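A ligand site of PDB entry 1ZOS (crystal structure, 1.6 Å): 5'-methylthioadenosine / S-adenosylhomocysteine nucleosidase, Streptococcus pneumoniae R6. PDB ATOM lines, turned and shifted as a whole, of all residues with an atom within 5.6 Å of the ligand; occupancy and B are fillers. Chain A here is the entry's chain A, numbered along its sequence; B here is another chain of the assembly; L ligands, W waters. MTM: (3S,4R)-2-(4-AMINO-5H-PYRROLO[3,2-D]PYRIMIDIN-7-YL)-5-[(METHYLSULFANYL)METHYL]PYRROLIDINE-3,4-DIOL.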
ATOM      1  N   ALA A   8      -9.601 -24.717  29.728  1.00  0.00           N
ATOM      2  CA  ALA A   8      -9.419 -26.125  29.412  1.00  0.00           C
ATOM      3  C   ALA A   8      -8.027 -26.665  29.733  1.00  0.00           C
ATOM      4  O   ALA A   8      -7.903 -27.781  30.239  1.00  0.00           O
ATOM      5  CB  ALA A   8      -9.738 -26.369  27.938  1.00  0.00           C
ATOM      6  N   MET A   9      -7.006 -25.880  29.451  1.00  0.00           N
ATOM      7  CA  MET A   9      -5.630 -26.293  29.676  1.00  0.00           C
ATOM      8  C   MET A   9      -4.859 -25.366  30.611  1.00  0.00           C
ATOM      9  O   MET A   9      -5.236 -24.210  30.821  1.00  0.00           O
ATOM     10  CB  MET A   9      -4.898 -26.375  28.330  1.00  0.00           C
ATOM     11  CG  MET A   9      -5.443 -27.469  27.413  1.00  0.00           C
ATOM     12  SD  MET A   9      -4.715 -27.409  25.765  1.00  0.00           S
ATOM     13  CE  MET A   9      -3.027 -27.928  26.104  1.00  0.00           C
ATOM     14  N   GLU A  12      -3.904 -21.799  29.703  1.00  0.00           N
ATOM     15  CA  GLU A  12      -4.985 -20.826  29.671  1.00  0.00           C
ATOM     16  C   GLU A  12      -5.417 -20.323  31.040  1.00  0.00           C
ATOM     17  O   GLU A  12      -6.226 -19.402  31.136  1.00  0.00           O
ATOM     18  CB  GLU A  12      -6.172 -21.437  28.917  1.00  0.00           C
ATOM     19  CG  GLU A  12      -5.794 -21.935  27.523  1.00  0.00           C
ATOM     20  CD  GLU A  12      -6.835 -22.852  26.906  1.00  0.00           C
ATOM     21  OE1 GLU A  12      -7.373 -23.713  27.623  1.00  0.00           O
ATOM     22  OE2 GLU A  12      -7.108 -22.730  25.689  1.00  0.00           O
ATOM     23  N   ILE A  50      -9.964 -30.799  28.436  1.00  0.00           N
ATOM     24  CA  ILE A  50     -10.542 -30.519  27.120  1.00  0.00           C
ATOM     25  C   ILE A  50     -11.870 -31.192  26.802  1.00  0.00           C
ATOM     26  O   ILE A  50     -12.107 -32.339  27.182  1.00  0.00           O
ATOM     27  CB  ILE A  50      -9.530 -30.899  26.027  1.00  0.00           C
ATOM     28  CG1 ILE A  50      -8.288 -30.003  26.159  1.00  0.00           C
ATOM     29  CG2 ILE A  50     -10.152 -30.778  24.640  1.00  0.00           C
ATOM     30  CD1 ILE A  50      -7.065 -30.570  25.485  1.00  0.00           C
ATOM     31  N   GLY A  51     -12.742 -30.470  26.099  1.00  0.00           N
ATOM     32  CA  GLY A  51     -13.996 -31.067  25.667  1.00  0.00           C
ATOM     33  C   GLY A  51     -15.275 -30.744  26.409  1.00  0.00           C
ATOM     34  O   GLY A  51     -15.265 -30.147  27.471  1.00  0.00           O
ATOM     35  N   SER A  76      -8.067 -20.610  24.275  1.00  0.00           N
ATOM     36  CA  SER A  76      -7.727 -20.516  22.865  1.00  0.00           C
ATOM     37  C   SER A  76      -8.842 -21.023  21.956  1.00  0.00           C
ATOM     38  O   SER A  76      -9.731 -21.758  22.401  1.00  0.00           O
ATOM     39  CB  SER A  76      -6.483 -21.350  22.577  1.00  0.00           C
ATOM     40  OG  SER A  76      -6.744 -22.717  22.881  1.00  0.00           O
ATOM     41  N   ALA A  77      -8.785 -20.633  20.693  1.00  0.00           N
ATOM     42  CA  ALA A  77      -9.762 -21.069  19.705  1.00  0.00           C
ATOM     43  C   ALA A  77      -9.158 -20.929  18.317  1.00  0.00           C
ATOM     44  O   ALA A  77      -8.107 -20.299  18.146  1.00  0.00           O
ATOM     45  CB  ALA A  77     -11.051 -20.248  19.809  1.00  0.00           C
ATOM     46  N   GLY A  78      -9.816 -21.540  17.327  1.00  0.00           N
ATOM     47  CA  GLY A  78      -9.334 -21.457  15.959  1.00  0.00           C
ATOM     48  C   GLY A  78     -10.085 -20.361  15.224  1.00  0.00           C
ATOM     49  O   GLY A  78     -11.314 -20.317  15.282  1.00  0.00           O
ATOM     50  N   SER A 150     -14.496 -31.634  18.563  1.00  0.00           N
ATOM     51  CA  SER A 150     -13.467 -31.930  17.570  1.00  0.00           C
ATOM     52  C   SER A 150     -12.528 -30.744  17.401  1.00  0.00           C
ATOM     53  O   SER A 150     -12.928 -29.597  17.563  1.00  0.00           O
ATOM     54  CB  SER A 150     -14.076 -32.235  16.199  1.00  0.00           C
ATOM     55  OG  SER A 150     -14.823 -33.452  16.192  1.00  0.00           O
ATOM     56  N   PHE A 151     -11.283 -31.043  17.062  1.00  0.00           N
ATOM     57  CA  PHE A 151     -10.312 -29.991  16.810  1.00  0.00           C
ATOM     58  C   PHE A 151     -10.409 -29.760  15.301  1.00  0.00           C
ATOM     59  O   PHE A 151     -10.095 -30.640  14.494  1.00  0.00           O
ATOM     60  CB  PHE A 151      -8.913 -30.449  17.200  1.00  0.00           C
ATOM     61  CG  PHE A 151      -7.836 -29.441  16.935  1.00  0.00           C
ATOM     62  CD1 PHE A 151      -7.008 -29.570  15.822  1.00  0.00           C
ATOM     63  CD2 PHE A 151      -7.654 -28.367  17.792  1.00  0.00           C
ATOM     64  CE1 PHE A 151      -6.002 -28.632  15.570  1.00  0.00           C
ATOM     65  CE2 PHE A 151      -6.654 -27.418  17.548  1.00  0.00           C
ATOM     66  CZ  PHE A 151      -5.822 -27.560  16.441  1.00  0.00           C
ATOM     67  N   VAL A 152     -10.871 -28.575  14.903  1.00  0.00           N
ATOM     68  CA  VAL A 152     -11.036 -28.244  13.494  1.00  0.00           C
ATOM     69  C   VAL A 152      -9.676 -27.949  12.857  1.00  0.00           C
ATOM     70  O   VAL A 152      -8.978 -27.029  13.276  1.00  0.00           O
ATOM     71  CB  VAL A 152     -11.977 -27.036  13.329  1.00  0.00           C
ATOM     72  CG1 VAL A 152     -12.246 -26.770  11.856  1.00  0.00           C
ATOM     73  CG2 VAL A 152     -13.283 -27.303  14.067  1.00  0.00           C
ATOM     74  N   ALA A 153      -9.325 -28.735  11.851  1.00  0.00           N
ATOM     75  CA  ALA A 153      -8.029 -28.565  11.187  1.00  0.00           C
ATOM     76  C   ALA A 153      -8.098 -28.851   9.686  1.00  0.00           C
ATOM     77  O   ALA A 153      -7.391 -29.716   9.163  1.00  0.00           O
ATOM     78  CB  ALA A 153      -7.009 -29.476  11.846  1.00  0.00           C
ATOM     79  N   VAL A 171     -13.821 -21.193  16.446  1.00  0.00           N
ATOM     80  CA  VAL A 171     -14.306 -22.493  16.888  1.00  0.00           C
ATOM     81  C   VAL A 171     -13.456 -23.058  18.006  1.00  0.00           C
ATOM     82  O   VAL A 171     -12.238 -22.857  18.041  1.00  0.00           O
ATOM     83  CB  VAL A 171     -14.316 -23.522  15.730  1.00  0.00           C
ATOM     84  CG1 VAL A 171     -15.321 -23.096  14.666  1.00  0.00           C
ATOM     85  CG2 VAL A 171     -12.924 -23.658  15.120  1.00  0.00           C
ATOM     86  N   GLU A 172     -14.097 -23.757  18.940  1.00  0.00           N
ATOM     87  CA  GLU A 172     -13.374 -24.376  20.040  1.00  0.00           C
ATOM     88  C   GLU A 172     -14.126 -25.596  20.541  1.00  0.00           C
ATOM     89  O   GLU A 172     -15.056 -26.064  19.884  1.00  0.00           O
ATOM     90  CB  GLU A 172     -13.089 -23.370  21.164  1.00  0.00           C
ATOM     91  CG  GLU A 172     -13.913 -22.100  21.147  1.00  0.00           C
ATOM     92  CD  GLU A 172     -15.082 -22.200  22.107  1.00  0.00           C
ATOM     93  OE1 GLU A 172     -15.789 -23.202  22.018  1.00  0.00           O
ATOM     94  OE2 GLU A 172     -15.276 -21.278  22.928  1.00  0.00           O
ATOM     95  N   MET A 173     -13.727 -26.112  21.712  1.00  0.00           N
ATOM     96  CA  MET A 173     -14.331 -27.340  22.227  1.00  0.00           C
ATOM     97  C   MET A 173     -15.035 -27.308  23.571  1.00  0.00           C
ATOM     98  O   MET A 173     -15.418 -28.357  24.086  1.00  0.00           O
ATOM     99  CB  MET A 173     -13.251 -28.433  22.236  1.00  0.00           C
ATOM    100  CG  MET A 173     -12.678 -28.733  20.862  1.00  0.00           C
ATOM    101  SD  MET A 173     -11.199 -29.794  20.890  1.00  0.00           S
ATOM    102  CE  MET A 173     -11.951 -31.370  21.296  1.00  0.00           C
ATOM    103  N   GLU A 174     -15.225 -26.126  24.149  1.00  0.00           N
ATOM    104  CA  GLU A 174     -15.892 -26.045  25.442  1.00  0.00           C
ATOM    105  C   GLU A 174     -16.889 -24.904  25.585  1.00  0.00           C
ATOM    106  O   GLU A 174     -17.752 -24.951  26.467  1.00  0.00           O
ATOM    107  CB  GLU A 174     -14.874 -25.890  26.579  1.00  0.00           C
ATOM    108  CG  GLU A 174     -13.832 -26.989  26.675  1.00  0.00           C
ATOM    109  CD  GLU A 174     -12.643 -26.771  25.770  1.00  0.00           C
ATOM    110  OE1 GLU A 174     -11.949 -27.765  25.461  1.00  0.00           O
ATOM    111  OE2 GLU A 174     -12.374 -25.615  25.376  1.00  0.00           O
ATOM    112  N   ARG A 193     -12.094 -15.939  23.988  1.00  0.00           N
ATOM    113  CA  ARG A 193     -11.055 -16.811  23.428  1.00  0.00           C
ATOM    114  C   ARG A 193     -10.074 -16.009  22.582  1.00  0.00           C
ATOM    115  O   ARG A 193     -10.470 -15.053  21.922  1.00  0.00           O
ATOM    116  CB  ARG A 193     -11.676 -17.890  22.534  1.00  0.00           C
ATOM    117  CG  ARG A 193     -12.627 -18.864  23.213  1.00  0.00           C
ATOM    118  CD  ARG A 193     -11.933 -19.707  24.266  1.00  0.00           C
ATOM    119  NE  ARG A 193     -12.805 -20.749  24.822  1.00  0.00           N
ATOM    120  CZ  ARG A 193     -12.782 -22.024  24.454  1.00  0.00           C
ATOM    121  NH1 ARG A 193     -11.923 -22.426  23.523  1.00  0.00           N
ATOM    122  NH2 ARG A 193     -13.590 -22.906  25.027  1.00  0.00           N
ATOM    123  N   SER A 196      -5.429 -19.164  18.485  1.00  0.00           N
ATOM    124  CA  SER A 196      -4.140 -19.862  18.534  1.00  0.00           C
ATOM    125  C   SER A 196      -3.781 -20.459  17.182  1.00  0.00           C
ATOM    126  O   SER A 196      -2.639 -20.878  16.967  1.00  0.00           O
ATOM    127  CB  SER A 196      -4.211 -20.992  19.581  1.00  0.00           C
ATOM    128  OG  SER A 196      -5.329 -21.845  19.341  1.00  0.00           O
ATOM    129  N   ASP A 197      -4.737 -20.476  16.256  1.00  0.00           N
ATOM    130  CA  ASP A 197      -4.506 -21.076  14.951  1.00  0.00           C
ATOM    131  C   ASP A 197      -5.611 -20.679  13.980  1.00  0.00           C
ATOM    132  O   ASP A 197      -6.558 -19.978  14.355  1.00  0.00           O
ATOM    133  CB  ASP A 197      -4.478 -22.598  15.106  1.00  0.00           C
ATOM    134  CG  ASP A 197      -5.765 -23.145  15.697  1.00  0.00           C
ATOM    135  OD1 ASP A 197      -6.728 -23.365  14.933  1.00  0.00           O
ATOM    136  OD2 ASP A 197      -5.814 -23.339  16.934  1.00  0.00           O
ATOM    137  N   ASN A 198      -5.500 -21.138  12.741  1.00  0.00           N
ATOM    138  CA  ASN A 198      -6.483 -20.824  11.704  1.00  0.00           C
ATOM    139  C   ASN A 198      -7.445 -21.971  11.387  1.00  0.00           C
ATOM    140  O   ASN A 198      -8.118 -21.956  10.354  1.00  0.00           O
ATOM    141  CB  ASN A 198      -5.755 -20.373  10.430  1.00  0.00           C
ATOM    142  CG  ASN A 198      -5.006 -19.076  10.629  1.00  0.00           C
ATOM    143  OD1 ASN A 198      -5.568 -18.075  11.067  1.00  0.00           O
ATOM    144  ND2 ASN A 198      -3.709 -19.083  10.313  1.00  0.00           N
ATOM    145  N   ALA A 199      -7.502 -22.961  12.272  1.00  0.00           N
ATOM    146  CA  ALA A 199      -8.406 -24.098  12.113  1.00  0.00           C
ATOM    147  C   ALA A 199      -8.300 -24.795  10.756  1.00  0.00           C
ATOM    148  O   ALA A 199      -9.271 -25.420  10.290  1.00  0.00           O
ATOM    149  CB  ALA A 199      -9.842 -23.651  12.352  1.00  0.00           C
ATOM    150  N   ALA A 203      -3.416 -26.242  11.585  1.00  0.00           N
ATOM    151  CA  ALA A 203      -3.895 -25.932  12.928  1.00  0.00           C
ATOM    152  C   ALA A 203      -3.175 -26.576  14.105  1.00  0.00           C
ATOM    153  O   ALA A 203      -2.957 -25.907  15.116  1.00  0.00           O
ATOM    154  CB  ALA A 203      -5.398 -26.219  13.022  1.00  0.00           C
ATOM    155  N   PHE A 207      -1.323 -24.345  16.852  1.00  0.00           N
ATOM    156  CA  PHE A 207      -1.780 -24.479  18.233  1.00  0.00           C
ATOM    157  C   PHE A 207      -0.592 -24.754  19.156  1.00  0.00           C
ATOM    158  O   PHE A 207      -0.460 -24.136  20.209  1.00  0.00           O
ATOM    159  CB  PHE A 207      -2.786 -25.626  18.372  1.00  0.00           C
ATOM    160  CG  PHE A 207      -3.271 -25.819  19.784  1.00  0.00           C
ATOM    161  CD1 PHE A 207      -4.250 -24.968  20.316  1.00  0.00           C
ATOM    162  CD2 PHE A 207      -2.698 -26.780  20.616  1.00  0.00           C
ATOM    163  CE1 PHE A 207      -4.638 -25.080  21.641  1.00  0.00           C
ATOM    164  CE2 PHE A 207      -3.088 -26.894  21.955  1.00  0.00           C
ATOM    165  CZ  PHE A 207      -4.051 -26.041  22.469  1.00  0.00           C
ATOM    166  N   ILE A 211      -0.284 -21.731  21.793  1.00  0.00           N
ATOM    167  CA  ILE A 211      -1.143 -21.941  22.954  1.00  0.00           C
ATOM    168  C   ILE A 211      -0.738 -21.087  24.162  1.00  0.00           C
ATOM    169  O   ILE A 211      -1.594 -20.522  24.837  1.00  0.00           O
ATOM    170  CB  ILE A 211      -1.217 -23.441  23.374  1.00  0.00           C
ATOM    171  CG1 ILE A 211      -2.119 -23.614  24.596  1.00  0.00           C
ATOM    172  CG2 ILE A 211       0.174 -23.989  23.664  1.00  0.00           C
ATOM    173  CD1 ILE A 211      -3.541 -23.097  24.404  1.00  0.00           C
ATOM    174  N   VAL B 102      -9.988 -35.483  16.838  1.00  0.00           N
ATOM    175  CA  VAL B 102      -8.846 -34.714  17.327  1.00  0.00           C
ATOM    176  C   VAL B 102      -7.631 -35.397  16.702  1.00  0.00           C
ATOM    177  O   VAL B 102      -6.521 -35.363  17.240  1.00  0.00           O
ATOM    178  CB  VAL B 102      -8.735 -34.766  18.868  1.00  0.00           C
ATOM    179  CG1 VAL B 102      -7.686 -33.770  19.351  1.00  0.00           C
ATOM    180  CG2 VAL B 102     -10.098 -34.445  19.513  1.00  0.00           C
ATOM    181  N   PHE B 105      -3.789 -34.162  16.022  1.00  0.00           N
ATOM    182  CA  PHE B 105      -2.716 -34.289  17.005  1.00  0.00           C
ATOM    183  C   PHE B 105      -2.190 -35.725  17.131  1.00  0.00           C
ATOM    184  O   PHE B 105      -1.301 -35.987  17.945  1.00  0.00           O
ATOM    185  CB  PHE B 105      -3.183 -33.800  18.380  1.00  0.00           C
ATOM    186  CG  PHE B 105      -3.330 -32.307  18.467  1.00  0.00           C
ATOM    187  CD1 PHE B 105      -2.209 -31.490  18.500  1.00  0.00           C
ATOM    188  CD2 PHE B 105      -4.587 -31.731  18.496  1.00  0.00           C
ATOM    189  CE1 PHE B 105      -2.338 -30.103  18.563  1.00  0.00           C
ATOM    190  CE2 PHE B 105      -4.724 -30.339  18.559  1.00  0.00           C
ATOM    191  CZ  PHE B 105      -3.604 -29.522  18.591  1.00  0.00           C
ATOM    192  N   ALA B 113      -9.159 -35.660  23.336  1.00  0.00           N
ATOM    193  CA  ALA B 113      -7.842 -35.274  23.820  1.00  0.00           C
ATOM    194  C   ALA B 113      -7.748 -35.567  25.321  1.00  0.00           C
ATOM    195  O   ALA B 113      -8.712 -35.349  26.056  1.00  0.00           O
ATOM    196  CB  ALA B 113      -7.623 -33.775  23.567  1.00  0.00           C
HETATM  197  CS  MTM L   1      -5.936 -29.869  22.041  1.00  0.00           C
HETATM  198  S5' MTM L   1      -7.684 -29.694  21.568  1.00  0.00           S
HETATM  199  C5' MTM L   1      -7.785 -27.882  21.376  1.00  0.00           C
HETATM  200  C4' MTM L   1      -8.131 -27.072  22.655  1.00  0.00           C
HETATM  201  N4' MTM L   1      -7.923 -25.635  22.370  1.00  0.00           N
HETATM  202  C2' MTM L   1     -10.258 -26.018  22.249  1.00  0.00           C
HETATM  203  O2' MTM L   1     -11.316 -25.329  22.986  1.00  0.00           O
HETATM  204  C3' MTM L   1      -9.577 -27.179  23.116  1.00  0.00           C
HETATM  205  O3' MTM L   1      -9.677 -26.870  24.564  1.00  0.00           O
HETATM  206  C1' MTM L   1      -9.134 -25.005  21.813  1.00  0.00           C
HETATM  207  C9  MTM L   1      -8.903 -24.853  20.229  1.00  0.00           C
HETATM  208  C8  MTM L   1      -7.917 -24.067  19.643  1.00  0.00           C
HETATM  209  N7  MTM L   1      -7.891 -24.093  18.330  1.00  0.00           N
HETATM  210  C5  MTM L   1      -8.916 -24.951  17.985  1.00  0.00           C
HETATM  211  C6  MTM L   1      -9.430 -25.441  16.726  1.00  0.00           C
HETATM  212  N6  MTM L   1      -8.896 -25.068  15.564  1.00  0.00           N
HETATM  213  N1  MTM L   1     -10.535 -26.334  16.760  1.00  0.00           N
HETATM  214  C2  MTM L   1     -11.074 -26.724  17.970  1.00  0.00           C
HETATM  215  N3  MTM L   1     -10.650 -26.324  19.200  1.00  0.00           N
HETATM  216  C4  MTM L   1      -9.570 -25.441  19.131  1.00  0.00           C
HETATM  217  O   HOH W   1      -7.020 -25.240  25.002  1.00  0.00           O
HETATM  218  O   HOH W   2      -9.775 -23.517  25.315  1.00  0.00           O
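Ala 8 touches the ligand. Ile 50 touches the ligand. Ala 77 touches the ligand. O of Ser 150 touches C2 of the ligand, 3.4 Å away. CE2 of Phe 151 touches C5 of the ligand (3.4 Å). O of Val 171 touches C4 of the ligand, 3.9 Å away. Glu 172 touches the ligand (CB to O2', 3.2 Å). Ser 196 touches the ligand. Ala 199 touches the ligand (CA to N6, 3.6 Å). Phe 207 touches the ligand (CE1 to N4', 3.4 Å). Phe 105 of chain B touches the ligand (CE2 to CS, 3.7 Å). Hydrophobic or aromatic side chains that line the ligand: Ala 8, Ile 50, Phe 151, Val 152, Val 171, Met 173, Ala 199, Phe 207 and Phe 105 of chain B. Of the 27 residues printed, 18 come within 4 Å of the ligand. The nearest printed residue that does not touch the ligand is Ala 203 (4.5 Å).
The side-chain carboxylate (OE2) of Glu 174 lies within salt-bridge range of the guanidinium group (NH2) of Arg 193 (3.0 Å). The side-chain carboxylate (OE1) of Glu 174 sits at hydrogen-bond distance from the backbone NH (N) of Gly 51 (2.9 Å). The side-chain carboxylate of Asp 197 sits at hydrogen-bond distance from the side-chain hydroxyl of Ser 196 (2.9 Å). The backbone NH (N) of Ala 199 lies within hydrogen-bond range of the side-chain carboxylate (OD1) of Asp 197 (2.8 Å). The guanidinium group of Arg 193 is in salt-bridge range of the side-chain carboxylate of Glu 172 (3.1 Å). The backbone NH (N) of Ser 76 lies within hydrogen-bond range of the side-chain carboxylate (OE2) of Glu 12 (2.7 Å). N of Gly 78 lies within hydrogen-bond range of O of Val 171. The backbone NH (N) of Ser 196 is in hydrogen-bond range of the backbone carbonyl oxygen (O) of Ala 77 (2.9 Å).
Water W1 lies within hydrogen-bond range of OE2 of Glu 12 (2.6 Å), N4' of the ligand (2.8 Å), SD of Met 9 (3.3 Å) and OG of Ser 76 (3.3 Å).
The side-chain carboxylate (OE1) of Glu 174 sits at hydrogen-bond distance from an oxygen (O3') of the ligand (2.6 Å). OD1 of Asp 197 is in salt-bridge range of N6 of the ligand, 2.8 Å away. The backbone NH (N) of Met 173 is in hydrogen-bond range of an oxygen (O2') of the ligand, 2.8 Å away. A nitrogen (N6) of the ligand is in hydrogen-bond range of the backbone carbonyl oxygen of Val 152 (3.0 Å). The guanidinium group (NH1) of Arg 193 sits at hydrogen-bond distance from an oxygen (O2') of the ligand, 3.0 Å away. N4' of the ligand is in hydrogen-bond range of OG of Ser 76, 3.2 Å away. N of Gly 78 sits close to N7 of the ligand, at 3.4 Å.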
